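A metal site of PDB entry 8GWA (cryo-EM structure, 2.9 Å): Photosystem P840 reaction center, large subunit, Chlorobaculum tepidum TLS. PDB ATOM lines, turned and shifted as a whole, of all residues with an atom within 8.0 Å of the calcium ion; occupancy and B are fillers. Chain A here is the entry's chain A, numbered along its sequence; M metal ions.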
ATOM      1  N   PHE A 362      14.916 -12.656  10.051  1.00  0.00           N
ATOM      2  CA  PHE A 362      15.345 -12.677   8.660  1.00  0.00           C
ATOM      3  C   PHE A 362      15.811 -11.261   8.318  1.00  0.00           C
ATOM      4  O   PHE A 362      14.993 -10.362   8.135  1.00  0.00           O
ATOM      5  CB  PHE A 362      14.194 -13.124   7.766  1.00  0.00           C
ATOM      6  CG  PHE A 362      14.565 -13.330   6.322  1.00  0.00           C
ATOM      7  CD1 PHE A 362      14.860 -12.259   5.492  1.00  0.00           C
ATOM      8  CD2 PHE A 362      14.597 -14.610   5.791  1.00  0.00           C
ATOM      9  CE1 PHE A 362      15.203 -12.466   4.174  1.00  0.00           C
ATOM     10  CE2 PHE A 362      14.930 -14.806   4.473  1.00  0.00           C
ATOM     11  CZ  PHE A 362      15.237 -13.735   3.662  1.00  0.00           C
ATOM     12  N   GLY A 363      17.129 -11.070   8.210  1.00  0.00           N
ATOM     13  CA  GLY A 363      17.653  -9.733   8.086  1.00  0.00           C
ATOM     14  C   GLY A 363      17.383  -9.096   6.740  1.00  0.00           C
ATOM     15  O   GLY A 363      18.307  -8.856   5.959  1.00  0.00           O
ATOM     16  N   ARG A 366      19.722  -6.111   5.285  1.00  0.00           N
ATOM     17  CA  ARG A 366      20.950  -6.489   4.622  1.00  0.00           C
ATOM     18  C   ARG A 366      20.741  -7.619   3.616  1.00  0.00           C
ATOM     19  O   ARG A 366      21.587  -7.811   2.756  1.00  0.00           O
ATOM     20  CB  ARG A 366      22.033  -6.858   5.629  1.00  0.00           C
ATOM     21  CG  ARG A 366      23.419  -6.949   5.001  1.00  0.00           C
ATOM     22  CD  ARG A 366      24.525  -6.391   5.876  1.00  0.00           C
ATOM     23  NE  ARG A 366      25.812  -6.962   5.516  1.00  0.00           N
ATOM     24  CZ  ARG A 366      26.897  -6.887   6.270  1.00  0.00           C
ATOM     25  NH1 ARG A 366      26.901  -6.246   7.421  1.00  0.00           N
ATOM     26  NH2 ARG A 366      28.020  -7.472   5.851  1.00  0.00           N
ATOM     27  N   VAL A 367      19.618  -8.347   3.678  1.00  0.00           N
ATOM     28  CA  VAL A 367      19.337  -9.306   2.622  1.00  0.00           C
ATOM     29  C   VAL A 367      19.124  -8.593   1.297  1.00  0.00           C
ATOM     30  O   VAL A 367      19.714  -8.946   0.273  1.00  0.00           O
ATOM     31  CB  VAL A 367      18.123 -10.185   2.983  1.00  0.00           C
ATOM     32  CG1 VAL A 367      17.562 -10.846   1.749  1.00  0.00           C
ATOM     33  CG2 VAL A 367      18.532 -11.238   3.994  1.00  0.00           C
ATOM     34  N   ASN A 370      22.459  -6.940   0.270  1.00  0.00           N
ATOM     35  CA  ASN A 370      23.378  -7.920  -0.307  1.00  0.00           C
ATOM     36  C   ASN A 370      22.915  -8.364  -1.686  1.00  0.00           C
ATOM     37  O   ASN A 370      23.737  -8.556  -2.584  1.00  0.00           O
ATOM     38  CB  ASN A 370      23.512  -9.125   0.621  1.00  0.00           C
ATOM     39  CG  ASN A 370      24.342  -8.821   1.850  1.00  0.00           C
ATOM     40  OD1 ASN A 370      24.888  -7.726   1.991  1.00  0.00           O
ATOM     41  ND2 ASN A 370      24.433  -9.793   2.750  1.00  0.00           N
ATOM     42  N   LEU A 371      21.604  -8.548  -1.874  1.00  0.00           N
ATOM     43  CA  LEU A 371      21.104  -8.905  -3.192  1.00  0.00           C
ATOM     44  C   LEU A 371      21.494  -7.858  -4.226  1.00  0.00           C
ATOM     45  O   LEU A 371      22.066  -8.179  -5.271  1.00  0.00           O
ATOM     46  CB  LEU A 371      19.585  -9.087  -3.156  1.00  0.00           C
ATOM     47  CG  LEU A 371      19.059 -10.396  -2.590  1.00  0.00           C
ATOM     48  CD1 LEU A 371      17.544 -10.439  -2.718  1.00  0.00           C
ATOM     49  CD2 LEU A 371      19.674 -11.588  -3.290  1.00  0.00           C
ATOM     50  N   CYS A 559      30.091 -12.962  -1.459  1.00  0.00           N
ATOM     51  CA  CYS A 559      28.858 -13.470  -0.860  1.00  0.00           C
ATOM     52  C   CYS A 559      29.086 -13.916   0.570  1.00  0.00           C
ATOM     53  O   CYS A 559      28.253 -13.641   1.454  1.00  0.00           O
ATOM     54  CB  CYS A 559      28.313 -14.631  -1.676  1.00  0.00           C
ATOM     55  SG  CYS A 559      26.849 -15.411  -0.949  1.00  0.00           S
ATOM     56  N   TRP A 560      30.188 -14.619   0.830  1.00  0.00           N
ATOM     57  CA  TRP A 560      30.558 -14.961   2.194  1.00  0.00           C
ATOM     58  C   TRP A 560      30.728 -13.691   3.043  1.00  0.00           C
ATOM     59  O   TRP A 560      30.238 -13.628   4.170  1.00  0.00           O
ATOM     60  CB  TRP A 560      31.848 -15.773   2.185  1.00  0.00           C
ATOM     61  CG  TRP A 560      31.685 -17.256   2.211  1.00  0.00           C
ATOM     62  CD1 TRP A 560      31.961 -18.097   3.251  1.00  0.00           C
ATOM     63  CD2 TRP A 560      31.211 -18.089   1.145  1.00  0.00           C
ATOM     64  NE1 TRP A 560      31.691 -19.396   2.903  1.00  0.00           N
ATOM     65  CE2 TRP A 560      31.235 -19.423   1.613  1.00  0.00           C
ATOM     66  CE3 TRP A 560      30.769 -17.846  -0.157  1.00  0.00           C
ATOM     67  CZ2 TRP A 560      30.829 -20.487   0.823  1.00  0.00           C
ATOM     68  CZ3 TRP A 560      30.369 -18.905  -0.939  1.00  0.00           C
ATOM     69  CH2 TRP A 560      30.401 -20.215  -0.450  1.00  0.00           C
ATOM     70  N   ILE A 562      29.668 -10.392   2.550  1.00  0.00           N
ATOM     71  CA  ILE A 562      28.518  -9.526   2.756  1.00  0.00           C
ATOM     72  C   ILE A 562      27.467 -10.198   3.628  1.00  0.00           C
ATOM     73  O   ILE A 562      26.618  -9.518   4.210  1.00  0.00           O
ATOM     74  CB  ILE A 562      27.919  -9.080   1.410  1.00  0.00           C
ATOM     75  CG1 ILE A 562      27.405 -10.271   0.617  1.00  0.00           C
ATOM     76  CG2 ILE A 562      28.953  -8.306   0.602  1.00  0.00           C
ATOM     77  CD1 ILE A 562      26.950  -9.914  -0.789  1.00  0.00           C
ATOM     78  N   ASP A 563      27.525 -11.517   3.744  1.00  0.00           N
ATOM     79  CA  ASP A 563      26.719 -12.255   4.703  1.00  0.00           C
ATOM     80  C   ASP A 563      27.411 -12.429   6.045  1.00  0.00           C
ATOM     81  O   ASP A 563      26.815 -13.008   6.964  1.00  0.00           O
ATOM     82  CB  ASP A 563      26.343 -13.625   4.141  1.00  0.00           C
ATOM     83  CG  ASP A 563      25.286 -13.544   3.065  1.00  0.00           C
ATOM     84  OD1 ASP A 563      24.497 -12.572   3.070  1.00  0.00           O
ATOM     85  OD2 ASP A 563      25.232 -14.459   2.214  1.00  0.00           O
ATOM     86  N   GLY A 564      28.653 -11.960   6.180  1.00  0.00           N
ATOM     87  CA  GLY A 564      29.410 -12.167   7.390  1.00  0.00           C
ATOM     88  C   GLY A 564      29.662 -13.635   7.660  1.00  0.00           C
ATOM     89  O   GLY A 564      29.034 -14.221   8.551  1.00  0.00           O
ATOM     90  N   THR A 593      28.428 -15.824  10.727  1.00  0.00           N
ATOM     91  CA  THR A 593      27.649 -17.041  10.593  1.00  0.00           C
ATOM     92  C   THR A 593      28.473 -18.292  10.908  1.00  0.00           C
ATOM     93  O   THR A 593      28.221 -18.964  11.910  1.00  0.00           O
ATOM     94  CB  THR A 593      27.087 -17.161   9.175  1.00  0.00           C
ATOM     95  OG1 THR A 593      28.159 -17.225   8.237  1.00  0.00           O
ATOM     96  CG2 THR A 593      26.216 -15.968   8.848  1.00  0.00           C
ATOM     97  N   TYR A 599      29.728 -22.752   6.538  1.00  0.00           N
ATOM     98  CA  TYR A 599      28.733 -21.872   5.937  1.00  0.00           C
ATOM     99  C   TYR A 599      27.670 -22.648   5.180  1.00  0.00           C
ATOM    100  O   TYR A 599      26.546 -22.151   5.026  1.00  0.00           O
ATOM    101  CB  TYR A 599      29.418 -20.886   4.991  1.00  0.00           C
ATOM    102  CG  TYR A 599      28.565 -19.737   4.520  1.00  0.00           C
ATOM    103  CD1 TYR A 599      27.880 -18.933   5.421  1.00  0.00           C
ATOM    104  CD2 TYR A 599      28.474 -19.439   3.173  1.00  0.00           C
ATOM    105  CE1 TYR A 599      27.113 -17.879   4.970  1.00  0.00           C
ATOM    106  CE2 TYR A 599      27.720 -18.382   2.724  1.00  0.00           C
ATOM    107  CZ  TYR A 599      27.035 -17.616   3.620  1.00  0.00           C
ATOM    108  OH  TYR A 599      26.276 -16.564   3.164  1.00  0.00           O
ATOM    109  N   GLU A 603      22.780 -21.451   8.087  1.00  0.00           N
ATOM    110  CA  GLU A 603      22.110 -20.590   7.108  1.00  0.00           C
ATOM    111  C   GLU A 603      21.619 -21.396   5.909  1.00  0.00           C
ATOM    112  O   GLU A 603      20.874 -20.888   5.071  1.00  0.00           O
ATOM    113  CB  GLU A 603      23.050 -19.448   6.687  1.00  0.00           C
ATOM    114  CG  GLU A 603      22.416 -18.368   5.826  1.00  0.00           C
ATOM    115  CD  GLU A 603      23.339 -17.193   5.613  1.00  0.00           C
ATOM    116  OE1 GLU A 603      24.459 -17.210   6.154  1.00  0.00           O
ATOM    117  OE2 GLU A 603      22.934 -16.251   4.899  1.00  0.00           O
ATOM    118  N   THR A 606      17.837 -22.559   6.799  1.00  0.00           N
ATOM    119  CA  THR A 606      16.695 -21.815   6.289  1.00  0.00           C
ATOM    120  C   THR A 606      16.454 -22.034   4.803  1.00  0.00           C
ATOM    121  O   THR A 606      15.311 -21.901   4.351  1.00  0.00           O
ATOM    122  CB  THR A 606      16.892 -20.316   6.555  1.00  0.00           C
ATOM    123  OG1 THR A 606      18.102 -19.872   5.929  1.00  0.00           O
ATOM    124  CG2 THR A 606      16.982 -20.060   8.053  1.00  0.00           C
ATOM    125  N   VAL A 689      24.445 -19.121  -4.808  1.00  0.00           N
ATOM    126  CA  VAL A 689      24.937 -17.934  -4.124  1.00  0.00           C
ATOM    127  C   VAL A 689      23.771 -17.003  -3.818  1.00  0.00           C
ATOM    128  O   VAL A 689      23.722 -16.376  -2.744  1.00  0.00           O
ATOM    129  CB  VAL A 689      26.024 -17.234  -4.970  1.00  0.00           C
ATOM    130  CG1 VAL A 689      26.409 -15.913  -4.356  1.00  0.00           C
ATOM    131  CG2 VAL A 689      27.247 -18.125  -5.090  1.00  0.00           C
ATOM    132  N   PHE A 690      22.796 -16.925  -4.728  1.00  0.00           N
ATOM    133  CA  PHE A 690      21.555 -16.221  -4.447  1.00  0.00           C
ATOM    134  C   PHE A 690      20.851 -16.809  -3.236  1.00  0.00           C
ATOM    135  O   PHE A 690      20.301 -16.065  -2.405  1.00  0.00           O
ATOM    136  CB  PHE A 690      20.655 -16.279  -5.676  1.00  0.00           C
ATOM    137  CG  PHE A 690      19.205 -16.017  -5.390  1.00  0.00           C
ATOM    138  CD1 PHE A 690      18.760 -14.742  -5.066  1.00  0.00           C
ATOM    139  CD2 PHE A 690      18.275 -17.040  -5.439  1.00  0.00           C
ATOM    140  CE1 PHE A 690      17.432 -14.497  -4.810  1.00  0.00           C
ATOM    141  CE2 PHE A 690      16.934 -16.806  -5.180  1.00  0.00           C
ATOM    142  CZ  PHE A 690      16.519 -15.533  -4.865  1.00  0.00           C
ATOM    143  N   LEU A 691      20.843 -18.129  -3.109  1.00  0.00           N
ATOM    144  CA  LEU A 691      20.215 -18.771  -1.968  1.00  0.00           C
ATOM    145  C   LEU A 691      20.925 -18.404  -0.667  1.00  0.00           C
ATOM    146  O   LEU A 691      20.272 -18.141   0.351  1.00  0.00           O
ATOM    147  CB  LEU A 691      20.191 -20.286  -2.148  1.00  0.00           C
ATOM    148  CG  LEU A 691      19.319 -20.738  -3.307  1.00  0.00           C
ATOM    149  CD1 LEU A 691      19.163 -22.234  -3.265  1.00  0.00           C
ATOM    150  CD2 LEU A 691      17.977 -20.055  -3.232  1.00  0.00           C
ATOM    151  N   PHE A 692      22.258 -18.377  -0.684  1.00  0.00           N
ATOM    152  CA  PHE A 692      22.972 -17.845   0.480  1.00  0.00           C
ATOM    153  C   PHE A 692      22.557 -16.415   0.768  1.00  0.00           C
ATOM    154  O   PHE A 692      22.433 -16.020   1.934  1.00  0.00           O
ATOM    155  CB  PHE A 692      24.489 -17.890   0.304  1.00  0.00           C
ATOM    156  CG  PHE A 692      25.116 -19.205   0.661  1.00  0.00           C
ATOM    157  CD1 PHE A 692      24.894 -19.770   1.913  1.00  0.00           C
ATOM    158  CD2 PHE A 692      26.026 -19.804  -0.179  1.00  0.00           C
ATOM    159  CE1 PHE A 692      25.501 -20.954   2.260  1.00  0.00           C
ATOM    160  CE2 PHE A 692      26.646 -20.986   0.170  1.00  0.00           C
ATOM    161  CZ  PHE A 692      26.381 -21.569   1.397  1.00  0.00           C
ATOM    162  N   LEU A 693      22.352 -15.615  -0.276  1.00  0.00           N
ATOM    163  CA  LEU A 693      22.036 -14.200  -0.073  1.00  0.00           C
ATOM    164  C   LEU A 693      20.574 -13.999   0.333  1.00  0.00           C
ATOM    165  O   LEU A 693      20.278 -13.145   1.175  1.00  0.00           O
ATOM    166  CB  LEU A 693      22.340 -13.419  -1.342  1.00  0.00           C
ATOM    167  CG  LEU A 693      23.833 -13.349  -1.658  1.00  0.00           C
ATOM    168  CD1 LEU A 693      24.061 -12.710  -3.005  1.00  0.00           C
ATOM    169  CD2 LEU A 693      24.570 -12.592  -0.569  1.00  0.00           C
ATOM    170  N   ALA A 694      19.653 -14.764  -0.244  1.00  0.00           N
ATOM    171  CA  ALA A 694      18.229 -14.531  -0.076  1.00  0.00           C
ATOM    172  C   ALA A 694      17.580 -15.363   1.016  1.00  0.00           C
ATOM    173  O   ALA A 694      16.368 -15.285   1.199  1.00  0.00           O
ATOM    174  CB  ALA A 694      17.493 -14.771  -1.393  1.00  0.00           C
ATOM    175  N   ASN A 695      18.351 -16.167   1.750  1.00  0.00           N
ATOM    176  CA  ASN A 695      17.783 -16.986   2.811  1.00  0.00           C
ATOM    177  C   ASN A 695      17.821 -16.307   4.169  1.00  0.00           C
ATOM    178  O   ASN A 695      17.309 -16.864   5.135  1.00  0.00           O
ATOM    179  CB  ASN A 695      18.496 -18.347   2.885  1.00  0.00           C
ATOM    180  CG  ASN A 695      19.946 -18.223   3.314  1.00  0.00           C
ATOM    181  OD1 ASN A 695      20.474 -17.125   3.482  1.00  0.00           O
ATOM    182  ND2 ASN A 695      20.598 -19.361   3.467  1.00  0.00           N
ATOM    183  N   GLY A 696      18.393 -15.114   4.255  1.00  0.00           N
ATOM    184  CA  GLY A 696      18.555 -14.410   5.512  1.00  0.00           C
ATOM    185  C   GLY A 696      19.978 -13.968   5.732  1.00  0.00           C
ATOM    186  O   GLY A 696      20.911 -14.378   5.041  1.00  0.00           O
ATOM    187  N   PHE A 697      20.145 -13.112   6.746  1.00  0.00           N
ATOM    188  CA  PHE A 697      21.470 -12.609   7.092  1.00  0.00           C
ATOM    189  C   PHE A 697      22.115 -13.476   8.167  1.00  0.00           C
ATOM    190  O   PHE A 697      23.188 -14.046   7.950  1.00  0.00           O
ATOM    191  CB  PHE A 697      21.353 -11.149   7.549  1.00  0.00           C
ATOM    192  CG  PHE A 697      22.682 -10.450   7.669  1.00  0.00           C
ATOM    193  CD1 PHE A 697      23.719 -10.749   6.809  1.00  0.00           C
ATOM    194  CD2 PHE A 697      22.885  -9.498   8.663  1.00  0.00           C
ATOM    195  CE1 PHE A 697      24.934 -10.108   6.927  1.00  0.00           C
ATOM    196  CE2 PHE A 697      24.101  -8.857   8.781  1.00  0.00           C
ATOM    197  CZ  PHE A 697      25.126  -9.165   7.907  1.00  0.00           C
ATOM    198  N   TYR A 698      21.468 -13.582   9.327  1.00  0.00           N
ATOM    199  CA  TYR A 698      21.892 -14.477  10.412  1.00  0.00           C
ATOM    200  C   TYR A 698      23.342 -14.204  10.818  1.00  0.00           C
ATOM    201  O   TYR A 698      24.138 -15.123  11.031  1.00  0.00           O
ATOM    202  CB  TYR A 698      21.698 -15.941  10.021  1.00  0.00           C
ATOM    203  CG  TYR A 698      20.373 -16.201   9.349  1.00  0.00           C
ATOM    204  CD1 TYR A 698      19.197 -15.664   9.855  1.00  0.00           C
ATOM    205  CD2 TYR A 698      20.298 -16.984   8.202  1.00  0.00           C
ATOM    206  CE1 TYR A 698      17.990 -15.901   9.245  1.00  0.00           C
ATOM    207  CE2 TYR A 698      19.086 -17.226   7.584  1.00  0.00           C
ATOM    208  CZ  TYR A 698      17.934 -16.677   8.106  1.00  0.00           C
ATOM    209  OH  TYR A 698      16.725 -16.908   7.508  1.00  0.00           O
ATOM    210  N   GLN A 699      23.660 -12.931  10.987  1.00  0.00           N
ATOM    211  CA  GLN A 699      25.005 -12.467  11.342  1.00  0.00           C
ATOM    212  C   GLN A 699      24.919 -11.630  12.614  1.00  0.00           C
ATOM    213  O   GLN A 699      25.342 -10.468  12.668  1.00  0.00           O
ATOM    214  CB  GLN A 699      25.629 -11.699  10.181  1.00  0.00           C
ATOM    215  CG  GLN A 699      27.141 -11.509  10.262  1.00  0.00           C
ATOM    216  CD  GLN A 699      27.535 -10.141  10.795  1.00  0.00           C
ATOM    217  OE1 GLN A 699      26.837  -9.158  10.577  1.00  0.00           O
ATOM    218  NE2 GLN A 699      28.666 -10.081  11.493  1.00  0.00           N
HETATM  219 CA    CA M   1      22.784 -14.268   3.534  1.00  0.00          CA
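The backbone carbonyl oxygen (O) of Phe 692 sits close to the side-chain amide oxygen (OD1) of Asn 695. The side-chain amide oxygen (OD1) of Asn 695 lies close to the side-chain carboxylate (OE2) of Glu 603, 3.0 Å away. The backbone carbonyl oxygen (O) of Glu 603 lies within hydrogen-bond range of the side-chain hydroxyl (OG1) of Thr 606, at 3.1 Å. OD1 of Asp 563 sits close to ND2 of Asn 370 (2.8 Å). The side-chain carboxylate (OD2) of Asp 563 lies close to the side-chain sulfur (SG) of Cys 559 (3.7 Å). The backbone carbonyl oxygen (O) of Leu 691 lies close to the side-chain amide oxygen (OD1) of Asn 695 (3.3 Å). The backbone carbonyl oxygen (O) of Asn 695 is in hydrogen-bond range of the side-chain hydroxyl (OH) of Tyr 698 (2.4 Å). O of Asn 695 sits at hydrogen-bond distance from OG1 of Thr 606 (3.2 Å).
Residues that only touch the calcium ion: Leu 693 and Asn 695. Six residues have an atom within 4 Å of the calcium ion: Asp 563, Glu 603, Phe 692, Leu 693, Asn 695 and Gly 696. The nearest printed residue that does not touch the calcium ion is Phe 697 (4.1 Å).
The calcium ion is bound by O of Phe 692 (2.4 Å), O of Gly 696 (2.4 Å), OE2 of Glu 603 (2.4 Å), OD1 of Asp 563 (2.5 Å) and OD2 of Asp 563 (2.8 Å). The calcium ion has five donor atoms within binding distance.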
